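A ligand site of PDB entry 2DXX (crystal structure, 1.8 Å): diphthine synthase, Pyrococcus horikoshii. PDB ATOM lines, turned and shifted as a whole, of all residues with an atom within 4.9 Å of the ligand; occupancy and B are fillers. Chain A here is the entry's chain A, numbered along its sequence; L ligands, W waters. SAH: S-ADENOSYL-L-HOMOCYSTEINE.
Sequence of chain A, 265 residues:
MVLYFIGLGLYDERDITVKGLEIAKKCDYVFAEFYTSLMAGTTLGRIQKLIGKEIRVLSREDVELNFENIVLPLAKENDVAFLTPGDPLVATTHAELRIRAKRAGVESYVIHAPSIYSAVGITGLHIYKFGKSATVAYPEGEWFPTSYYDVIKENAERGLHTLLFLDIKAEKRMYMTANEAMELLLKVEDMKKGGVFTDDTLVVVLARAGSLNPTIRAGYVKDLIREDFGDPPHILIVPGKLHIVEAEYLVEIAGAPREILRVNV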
ATOM      1  N   LEU A  10     -31.770  17.357 -25.399  1.00  0.00           N
ATOM      2  CA  LEU A  10     -30.781  17.980 -26.269  1.00  0.00           C
ATOM      3  C   LEU A  10     -30.984  19.290 -27.011  1.00  0.00           C
ATOM      4  O   LEU A  10     -30.094  20.132 -27.042  1.00  0.00           O
ATOM      5  CB  LEU A  10     -30.362  16.957 -27.327  1.00  0.00           C
ATOM      6  CG  LEU A  10     -29.856  15.591 -26.873  1.00  0.00           C
ATOM      7  CD1 LEU A  10     -29.965  14.601 -28.023  1.00  0.00           C
ATOM      8  CD2 LEU A  10     -28.429  15.725 -26.406  1.00  0.00           C
ATOM      9  N   TYR A  11     -32.152  19.458 -27.628  1.00  0.00           N
ATOM     10  CA  TYR A  11     -32.353  20.613 -28.483  1.00  0.00           C
ATOM     11  C   TYR A  11     -33.606  21.467 -28.290  1.00  0.00           C
ATOM     12  O   TYR A  11     -33.509  22.694 -28.209  1.00  0.00           O
ATOM     13  CB  TYR A  11     -32.269  20.098 -29.917  1.00  0.00           C
ATOM     14  CG  TYR A  11     -32.344  21.152 -30.990  1.00  0.00           C
ATOM     15  CD1 TYR A  11     -31.289  22.029 -31.207  1.00  0.00           C
ATOM     16  CD2 TYR A  11     -33.468  21.236 -31.817  1.00  0.00           C
ATOM     17  CE1 TYR A  11     -31.346  22.979 -32.227  1.00  0.00           C
ATOM     18  CE2 TYR A  11     -33.536  22.178 -32.839  1.00  0.00           C
ATOM     19  CZ  TYR A  11     -32.479  23.045 -33.034  1.00  0.00           C
ATOM     20  OH  TYR A  11     -32.543  23.975 -34.043  1.00  0.00           O
ATOM     21  N   THR A  36     -26.075  25.214 -17.597  1.00  0.00           N
ATOM     22  CA  THR A  36     -25.201  24.058 -17.775  1.00  0.00           C
ATOM     23  C   THR A  36     -25.077  23.657 -19.238  1.00  0.00           C
ATOM     24  O   THR A  36     -24.111  22.998 -19.626  1.00  0.00           O
ATOM     25  CB  THR A  36     -25.676  22.832 -16.972  1.00  0.00           C
ATOM     26  OG1 THR A  36     -27.031  22.523 -17.323  1.00  0.00           O
ATOM     27  CG2 THR A  36     -25.573  23.087 -15.479  1.00  0.00           C
ATOM     28  N   SER A  37     -26.050  24.058 -20.048  1.00  0.00           N
ATOM     29  CA  SER A  37     -26.026  23.739 -21.471  1.00  0.00           C
ATOM     30  C   SER A  37     -26.936  24.659 -22.261  1.00  0.00           C
ATOM     31  O   SER A  37     -27.668  25.468 -21.697  1.00  0.00           O
ATOM     32  CB  SER A  37     -26.434  22.286 -21.692  1.00  0.00           C
ATOM     33  OG  SER A  37     -26.257  21.928 -23.051  1.00  0.00           O
ATOM     34  N   LEU A  38     -26.894  24.522 -23.589  1.00  0.00           N
ATOM     35  CA  LEU A  38     -27.715  25.340 -24.461  1.00  0.00           C
ATOM     36  C   LEU A  38     -28.699  24.510 -25.287  1.00  0.00           C
ATOM     37  O   LEU A  38     -28.302  23.601 -26.006  1.00  0.00           O
ATOM     38  CB  LEU A  38     -26.834  26.156 -25.416  1.00  0.00           C
ATOM     39  CG  LEU A  38     -27.547  27.011 -26.459  1.00  0.00           C
ATOM     40  CD1 LEU A  38     -28.291  28.151 -25.777  1.00  0.00           C
ATOM     41  CD2 LEU A  38     -26.528  27.553 -27.450  1.00  0.00           C
ATOM     42  N   PRO A  85     -31.233  21.286 -18.931  1.00  0.00           N
ATOM     43  CA  PRO A  85     -31.050  20.855 -20.324  1.00  0.00           C
ATOM     44  C   PRO A  85     -30.434  19.449 -20.284  1.00  0.00           C
ATOM     45  O   PRO A  85     -29.841  19.065 -19.277  1.00  0.00           O
ATOM     46  CB  PRO A  85     -30.053  21.880 -20.869  1.00  0.00           C
ATOM     47  CG  PRO A  85     -29.987  23.058 -19.962  1.00  0.00           C
ATOM     48  CD  PRO A  85     -30.482  22.519 -18.654  1.00  0.00           C
ATOM     49  N   GLY A  86     -30.567  18.698 -21.375  1.00  0.00           N
ATOM     50  CA  GLY A  86     -30.017  17.344 -21.440  1.00  0.00           C
ATOM     51  C   GLY A  86     -30.442  16.462 -20.275  1.00  0.00           C
ATOM     52  O   GLY A  86     -31.598  16.486 -19.870  1.00  0.00           O
ATOM     53  N   ASP A  87     -29.518  15.667 -19.750  1.00  0.00           N
ATOM     54  CA  ASP A  87     -29.817  14.822 -18.595  1.00  0.00           C
ATOM     55  C   ASP A  87     -29.309  15.632 -17.408  1.00  0.00           C
ATOM     56  O   ASP A  87     -28.186  16.133 -17.413  1.00  0.00           O
ATOM     57  CB  ASP A  87     -29.074  13.479 -18.702  1.00  0.00           C
ATOM     58  CG  ASP A  87     -29.338  12.587 -17.514  1.00  0.00           C
ATOM     59  OD1 ASP A  87     -28.909  12.942 -16.397  1.00  0.00           O
ATOM     60  OD2 ASP A  87     -29.967  11.525 -17.698  1.00  0.00           O
ATOM     61  N   VAL A  90     -25.620  14.665 -15.901  1.00  0.00           N
ATOM     62  CA  VAL A  90     -24.491  14.443 -16.795  1.00  0.00           C
ATOM     63  C   VAL A  90     -23.681  15.725 -17.025  1.00  0.00           C
ATOM     64  O   VAL A  90     -24.188  16.692 -17.565  1.00  0.00           O
ATOM     65  CB  VAL A  90     -24.950  13.905 -18.156  1.00  0.00           C
ATOM     66  CG1 VAL A  90     -23.772  13.814 -19.131  1.00  0.00           C
ATOM     67  CG2 VAL A  90     -25.594  12.538 -17.969  1.00  0.00           C
ATOM     68  N   ALA A  91     -22.415  15.706 -16.622  1.00  0.00           N
ATOM     69  CA  ALA A  91     -21.532  16.843 -16.800  1.00  0.00           C
ATOM     70  C   ALA A  91     -22.043  18.090 -16.085  1.00  0.00           C
ATOM     71  O   ALA A  91     -21.871  19.219 -16.557  1.00  0.00           O
ATOM     72  CB  ALA A  91     -21.339  17.131 -18.296  1.00  0.00           C
ATOM     73  N   THR A  92     -22.703  17.867 -14.948  1.00  0.00           N
ATOM     74  CA  THR A  92     -23.140  18.900 -14.041  1.00  0.00           C
ATOM     75  C   THR A  92     -22.753  18.485 -12.630  1.00  0.00           C
ATOM     76  O   THR A  92     -22.272  17.384 -12.389  1.00  0.00           O
ATOM     77  CB  THR A  92     -24.681  19.041 -14.143  1.00  0.00           C
ATOM     78  OG1 THR A  92     -25.298  17.964 -13.441  1.00  0.00           O
ATOM     79  CG2 THR A  92     -25.129  19.019 -15.601  1.00  0.00           C
ATOM     80  N   PRO A 114     -32.534  12.610 -23.096  1.00  0.00           N
ATOM     81  CA  PRO A 114     -31.377  12.403 -23.964  1.00  0.00           C
ATOM     82  C   PRO A 114     -30.221  13.343 -23.598  1.00  0.00           C
ATOM     83  O   PRO A 114     -30.428  14.532 -23.326  1.00  0.00           O
ATOM     84  CB  PRO A 114     -31.929  12.627 -25.374  1.00  0.00           C
ATOM     85  CG  PRO A 114     -33.325  13.182 -25.292  1.00  0.00           C
ATOM     86  CD  PRO A 114     -33.750  12.886 -23.879  1.00  0.00           C
ATOM     87  N   SER A 115     -29.021  12.789 -23.588  1.00  0.00           N
ATOM     88  CA  SER A 115     -27.810  13.515 -23.223  1.00  0.00           C
ATOM     89  C   SER A 115     -26.785  13.512 -24.349  1.00  0.00           C
ATOM     90  O   SER A 115     -26.707  12.564 -25.120  1.00  0.00           O
ATOM     91  CB  SER A 115     -27.190  12.855 -21.981  1.00  0.00           C
ATOM     92  OG  SER A 115     -25.888  13.357 -21.720  1.00  0.00           O
ATOM     93  N   ILE A 116     -25.976  14.563 -24.438  1.00  0.00           N
ATOM     94  CA  ILE A 116     -24.971  14.628 -25.481  1.00  0.00           C
ATOM     95  C   ILE A 116     -23.959  13.492 -25.312  1.00  0.00           C
ATOM     96  O   ILE A 116     -23.362  13.028 -26.281  1.00  0.00           O
ATOM     97  CB  ILE A 116     -24.239  15.993 -25.457  1.00  0.00           C
ATOM     98  CG1 ILE A 116     -23.320  16.112 -26.683  1.00  0.00           C
ATOM     99  CG2 ILE A 116     -23.440  16.135 -24.184  1.00  0.00           C
ATOM    100  CD1 ILE A 116     -24.064  16.060 -28.010  1.00  0.00           C
ATOM    101  N   TYR A 117     -23.771  13.042 -24.077  1.00  0.00           N
ATOM    102  CA  TYR A 117     -22.826  11.983 -23.766  1.00  0.00           C
ATOM    103  C   TYR A 117     -23.129  10.702 -24.542  1.00  0.00           C
ATOM    104  O   TYR A 117     -22.210   9.981 -24.959  1.00  0.00           O
ATOM    105  CB  TYR A 117     -22.814  11.736 -22.260  1.00  0.00           C
ATOM    106  CG  TYR A 117     -21.833  10.694 -21.765  1.00  0.00           C
ATOM    107  CD1 TYR A 117     -20.461  10.888 -21.889  1.00  0.00           C
ATOM    108  CD2 TYR A 117     -22.288   9.533 -21.137  1.00  0.00           C
ATOM    109  CE1 TYR A 117     -19.558   9.944 -21.390  1.00  0.00           C
ATOM    110  CE2 TYR A 117     -21.404   8.592 -20.644  1.00  0.00           C
ATOM    111  CZ  TYR A 117     -20.040   8.808 -20.761  1.00  0.00           C
ATOM    112  OH  TYR A 117     -19.175   7.862 -20.241  1.00  0.00           O
ATOM    113  N   PHE A 165     -16.326  18.129 -24.134  1.00  0.00           N
ATOM    114  CA  PHE A 165     -17.425  19.045 -23.884  1.00  0.00           C
ATOM    115  C   PHE A 165     -16.792  20.425 -24.095  1.00  0.00           C
ATOM    116  O   PHE A 165     -15.616  20.616 -23.752  1.00  0.00           O
ATOM    117  CB  PHE A 165     -17.905  18.946 -22.438  1.00  0.00           C
ATOM    118  CG  PHE A 165     -18.562  17.635 -22.092  1.00  0.00           C
ATOM    119  CD1 PHE A 165     -19.915  17.429 -22.347  1.00  0.00           C
ATOM    120  CD2 PHE A 165     -17.831  16.615 -21.489  1.00  0.00           C
ATOM    121  CE1 PHE A 165     -20.539  16.235 -22.001  1.00  0.00           C
ATOM    122  CE2 PHE A 165     -18.450  15.409 -21.131  1.00  0.00           C
ATOM    123  CZ  PHE A 165     -19.798  15.223 -21.385  1.00  0.00           C
ATOM    124  N   LEU A 166     -17.534  21.366 -24.644  1.00  0.00           N
ATOM    125  CA  LEU A 166     -16.998  22.703 -24.879  1.00  0.00           C
ATOM    126  C   LEU A 166     -17.575  23.695 -23.881  1.00  0.00           C
ATOM    127  O   LEU A 166     -18.713  23.552 -23.429  1.00  0.00           O
ATOM    128  CB  LEU A 166     -17.270  23.126 -26.321  1.00  0.00           C
ATOM    129  CG  LEU A 166     -16.737  22.122 -27.361  1.00  0.00           C
ATOM    130  CD1 LEU A 166     -16.919  22.691 -28.759  1.00  0.00           C
ATOM    131  CD2 LEU A 166     -15.263  21.804 -27.108  1.00  0.00           C
ATOM    132  N   ASP A 167     -16.784  24.697 -23.525  1.00  0.00           N
ATOM    133  CA  ASP A 167     -17.168  25.701 -22.529  1.00  0.00           C
ATOM    134  C   ASP A 167     -18.405  26.531 -22.859  1.00  0.00           C
ATOM    135  O   ASP A 167     -18.785  26.706 -24.012  1.00  0.00           O
ATOM    136  CB  ASP A 167     -15.984  26.644 -22.259  1.00  0.00           C
ATOM    137  CG  ASP A 167     -15.922  27.099 -20.823  1.00  0.00           C
ATOM    138  OD1 ASP A 167     -16.847  26.789 -20.042  1.00  0.00           O
ATOM    139  OD2 ASP A 167     -14.939  27.788 -20.464  1.00  0.00           O
ATOM    140  N   ILE A 168     -19.030  27.034 -21.798  1.00  0.00           N
ATOM    141  CA  ILE A 168     -20.217  27.869 -21.928  1.00  0.00           C
ATOM    142  C   ILE A 168     -20.250  28.897 -20.809  1.00  0.00           C
ATOM    143  O   ILE A 168     -19.938  28.593 -19.654  1.00  0.00           O
ATOM    144  CB  ILE A 168     -21.515  27.016 -21.882  1.00  0.00           C
ATOM    145  CG1 ILE A 168     -22.737  27.942 -21.863  1.00  0.00           C
ATOM    146  CG2 ILE A 168     -21.516  26.123 -20.654  1.00  0.00           C
ATOM    147  CD1 ILE A 168     -24.072  27.208 -21.866  1.00  0.00           C
ATOM    148  N   LEU A 206     -19.878  17.548 -33.805  1.00  0.00           N
ATOM    149  CA  LEU A 206     -21.313  17.315 -33.748  1.00  0.00           C
ATOM    150  C   LEU A 206     -21.938  18.592 -33.210  1.00  0.00           C
ATOM    151  O   LEU A 206     -21.629  19.022 -32.100  1.00  0.00           O
ATOM    152  CB  LEU A 206     -21.646  16.135 -32.816  1.00  0.00           C
ATOM    153  CG  LEU A 206     -23.137  15.865 -32.584  1.00  0.00           C
ATOM    154  CD1 LEU A 206     -23.851  15.643 -33.912  1.00  0.00           C
ATOM    155  CD2 LEU A 206     -23.301  14.631 -31.686  1.00  0.00           C
ATOM    156  N   ALA A 207     -22.781  19.222 -34.022  1.00  0.00           N
ATOM    157  CA  ALA A 207     -23.429  20.460 -33.612  1.00  0.00           C
ATOM    158  C   ALA A 207     -24.947  20.355 -33.586  1.00  0.00           C
ATOM    159  O   ALA A 207     -25.555  19.834 -34.521  1.00  0.00           O
ATOM    160  CB  ALA A 207     -23.000  21.590 -34.545  1.00  0.00           C
ATOM    161  N   ARG A 208     -25.527  20.838 -32.511  1.00  0.00           N
ATOM    162  CA  ARG A 208     -26.978  20.834 -32.319  1.00  0.00           C
ATOM    163  C   ARG A 208     -27.580  19.434 -32.378  1.00  0.00           C
ATOM    164  O   ARG A 208     -28.558  19.185 -33.089  1.00  0.00           O
ATOM    165  CB  ARG A 208     -27.626  21.758 -33.360  1.00  0.00           C
ATOM    166  CG  ARG A 208     -27.097  23.194 -33.313  1.00  0.00           C
ATOM    167  CD  ARG A 208     -27.718  24.060 -34.415  1.00  0.00           C
ATOM    168  NE  ARG A 208     -27.603  23.409 -35.717  1.00  0.00           N
ATOM    169  CZ  ARG A 208     -26.467  23.272 -36.388  1.00  0.00           C
ATOM    170  NH1 ARG A 208     -25.332  23.750 -35.890  1.00  0.00           N
ATOM    171  NH2 ARG A 208     -26.456  22.624 -37.542  1.00  0.00           N
ATOM    172  N   ALA A 209     -26.976  18.513 -31.629  1.00  0.00           N
ATOM    173  CA  ALA A 209     -27.490  17.148 -31.563  1.00  0.00           C
ATOM    174  C   ALA A 209     -28.920  17.289 -31.044  1.00  0.00           C
ATOM    175  O   ALA A 209     -29.211  18.199 -30.254  1.00  0.00           O
ATOM    176  CB  ALA A 209     -26.647  16.317 -30.590  1.00  0.00           C
ATOM    177  N   GLY A 210     -29.825  16.410 -31.471  1.00  0.00           N
ATOM    178  CA  GLY A 210     -31.195  16.498 -31.015  1.00  0.00           C
ATOM    179  C   GLY A 210     -32.073  17.130 -32.075  1.00  0.00           C
ATOM    180  O   GLY A 210     -33.268  16.815 -32.176  1.00  0.00           O
ATOM    181  N   PRO A 233     -25.139  24.632 -29.686  1.00  0.00           N
ATOM    182  CA  PRO A 233     -23.903  24.123 -29.099  1.00  0.00           C
ATOM    183  C   PRO A 233     -23.149  23.129 -29.976  1.00  0.00           C
ATOM    184  O   PRO A 233     -23.737  22.504 -30.866  1.00  0.00           O
ATOM    185  CB  PRO A 233     -24.389  23.501 -27.803  1.00  0.00           C
ATOM    186  CG  PRO A 233     -25.715  22.930 -28.210  1.00  0.00           C
ATOM    187  CD  PRO A 233     -26.324  24.044 -29.037  1.00  0.00           C
ATOM    188  N   HIS A 234     -21.849  23.009 -29.722  1.00  0.00           N
ATOM    189  CA  HIS A 234     -20.970  22.105 -30.457  1.00  0.00           C
ATOM    190  C   HIS A 234     -20.226  21.223 -29.466  1.00  0.00           C
ATOM    191  O   HIS A 234     -20.036  21.596 -28.311  1.00  0.00           O
ATOM    192  CB  HIS A 234     -19.861  22.870 -31.202  1.00  0.00           C
ATOM    193  CG  HIS A 234     -20.331  23.777 -32.287  1.00  0.00           C
ATOM    194  ND1 HIS A 234     -19.455  24.516 -33.051  1.00  0.00           N
ATOM    195  CD2 HIS A 234     -21.572  24.066 -32.746  1.00  0.00           C
ATOM    196  CE1 HIS A 234     -20.134  25.214 -33.949  1.00  0.00           C
ATOM    197  NE2 HIS A 234     -21.412  24.961 -33.786  1.00  0.00           N
ATOM    198  N   ILE A 235     -19.789  20.056 -29.938  1.00  0.00           N
ATOM    199  CA  ILE A 235     -18.936  19.189 -29.137  1.00  0.00           C
ATOM    200  C   ILE A 235     -17.864  18.762 -30.115  1.00  0.00           C
ATOM    201  O   ILE A 235     -18.114  18.666 -31.317  1.00  0.00           O
ATOM    202  CB  ILE A 235     -19.613  17.917 -28.581  1.00  0.00           C
ATOM    203  CG1 ILE A 235     -20.294  17.143 -29.693  1.00  0.00           C
ATOM    204  CG2 ILE A 235     -20.550  18.289 -27.480  1.00  0.00           C
ATOM    205  CD1 ILE A 235     -20.460  15.683 -29.392  1.00  0.00           C
HETATM  206  N   SAH L   1     -26.268  17.609 -18.854  1.00  0.00           N
HETATM  207  CA  SAH L   1     -25.968  17.969 -20.305  1.00  0.00           C
HETATM  208  CB  SAH L   1     -24.556  18.366 -20.620  1.00  0.00           C
HETATM  209  CG  SAH L   1     -23.951  19.555 -19.891  1.00  0.00           C
HETATM  210  SD  SAH L   1     -22.316  19.888 -20.660  1.00  0.00           S
HETATM  211  C   SAH L   1     -26.378  16.708 -21.174  1.00  0.00           C
HETATM  212  O   SAH L   1     -26.821  15.696 -20.596  1.00  0.00           O
HETATM  213  OXT SAH L   1     -26.227  16.815 -22.460  1.00  0.00           O
HETATM  214  C5' SAH L   1     -22.779  21.109 -21.818  1.00  0.00           C
HETATM  215  C4' SAH L   1     -21.881  20.996 -23.126  1.00  0.00           C
HETATM  216  O4' SAH L   1     -22.233  19.748 -23.783  1.00  0.00           O
HETATM  217  C3' SAH L   1     -22.100  22.070 -24.125  1.00  0.00           C
HETATM  218  O3' SAH L   1     -21.293  23.210 -23.847  1.00  0.00           O
HETATM  219  C2' SAH L   1     -21.763  21.334 -25.444  1.00  0.00           C
HETATM  220  O2' SAH L   1     -20.350  21.293 -25.685  1.00  0.00           O
HETATM  221  C1' SAH L   1     -22.381  19.941 -25.259  1.00  0.00           C
HETATM  222  N9  SAH L   1     -23.680  19.835 -25.631  1.00  0.00           N
HETATM  223  C8  SAH L   1     -24.883  19.812 -24.945  1.00  0.00           C
HETATM  224  N7  SAH L   1     -25.935  19.670 -25.694  1.00  0.00           N
HETATM  225  C5  SAH L   1     -25.419  19.591 -27.014  1.00  0.00           C
HETATM  226  C6  SAH L   1     -26.084  19.423 -28.291  1.00  0.00           C
HETATM  227  N6  SAH L   1     -27.408  19.316 -28.430  1.00  0.00           N
HETATM  228  N1  SAH L   1     -25.244  19.387 -29.381  1.00  0.00           N
HETATM  229  C2  SAH L   1     -23.889  19.487 -29.284  1.00  0.00           C
HETATM  230  N3  SAH L   1     -23.224  19.644 -28.089  1.00  0.00           N
HETATM  231  C4  SAH L   1     -24.052  19.687 -26.997  1.00  0.00           C
HETATM  232  O   HOH W   1     -21.196  25.567 -25.385  1.00  0.00           O
HETATM  233  O   HOH W   2     -27.958  18.639 -23.878  1.00  0.00           O
HETATM  234  O   HOH W   3     -27.373  20.070 -18.460  1.00  0.00           O
HETATM  235  O   HOH W   4     -28.716  20.976 -24.201  1.00  0.00           O
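The side-chain hydroxyl of Ser 115 lies close to the backbone NH of Tyr 117 (3.2 Å). The backbone carbonyl oxygen (O) of Leu 206 is in hydrogen-bond range of the backbone NH (N) of Ile 235, 3.0 Å away. The backbone NH (N) of Arg 208 is in hydrogen-bond range of the backbone carbonyl oxygen (O) of Pro 233 (2.9 Å).
O of Val 90 sits at hydrogen-bond distance from N of the ligand, 2.6 Å away. An oxygen (O2') of the ligand is in hydrogen-bond range of the backbone NH of Leu 166 (3.0 Å). The backbone carbonyl oxygen of Leu 166 lies within hydrogen-bond range of an oxygen (O3') of the ligand. The backbone carbonyl oxygen (O) of His 234 lies within hydrogen-bond range of an oxygen (O2') of the ligand. O of the ligand lies within hydrogen-bond range of OG of Ser 115 (2.8 Å). The backbone NH (N) of Ala 209 lies within hydrogen-bond range of a nitrogen (N1) of the ligand (3.0 Å). A nitrogen (N6) of the ligand lies within hydrogen-bond range of the backbone carbonyl oxygen (O) of Ala 209 (2.8 Å). The backbone NH (N) of Asp 87 is in hydrogen-bond range of an oxygen (O) of the ligand (2.8 Å). The backbone carbonyl oxygen (O) of Asp 87 lies within hydrogen-bond range of a nitrogen (N) of the ligand. The backbone NH (N) of Ile 116 lies within hydrogen-bond range of an oxygen (OXT) of the ligand, at 3.0 Å. The backbone carbonyl oxygen of Leu 10 sits at hydrogen-bond distance from a nitrogen (N6) of the ligand (3.1 Å). OG of Ser 37 sits close to N7 of the ligand (3.5 Å). The backbone NH (N) of Arg 208 lies within hydrogen-bond range of a nitrogen (N1) of the ligand (3.5 Å).
Water W3 lies within hydrogen-bond range of the side-chain hydroxyl of Thr 36, a nitrogen (N) of the ligand and the backbone carbonyl oxygen of Pro 85. Water W1 bridges O3' of the ligand (2.8 Å) and O of Asp 167 (3.0 Å).
The backbone carbonyl oxygen (O) of Thr 36 sits close to a sulfur (SD) of the ligand. Pro 85 touches the ligand (O to N, 3.9 Å). Gly 86 touches the ligand (CA to O, 3.7 Å). Ala 91 touches the ligand (CB to SD, 3.8 Å). CG2 of Thr 92 touches N of the ligand, at 3.7 Å. Phe 165 touches the ligand (CD1 to O4', 3.6 Å). O of Leu 206 touches C2 of the ligand (3.6 Å). Pro 233 touches the ligand (O to C2, 3.4 Å). Ile 235 touches the ligand (CG2 to N3, 3.1 Å). 19 residues have an atom within 4 Å of the ligand: Leu 10, Thr 36, Ser 37, Pro 85, Gly 86, Asp 87, Val 90, Ala 91, Thr 92, Ser 115, Ile 116, Phe 165, Leu 166, Leu 206, Arg 208, Ala 209, Pro 233, His 234 and Ile 235.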
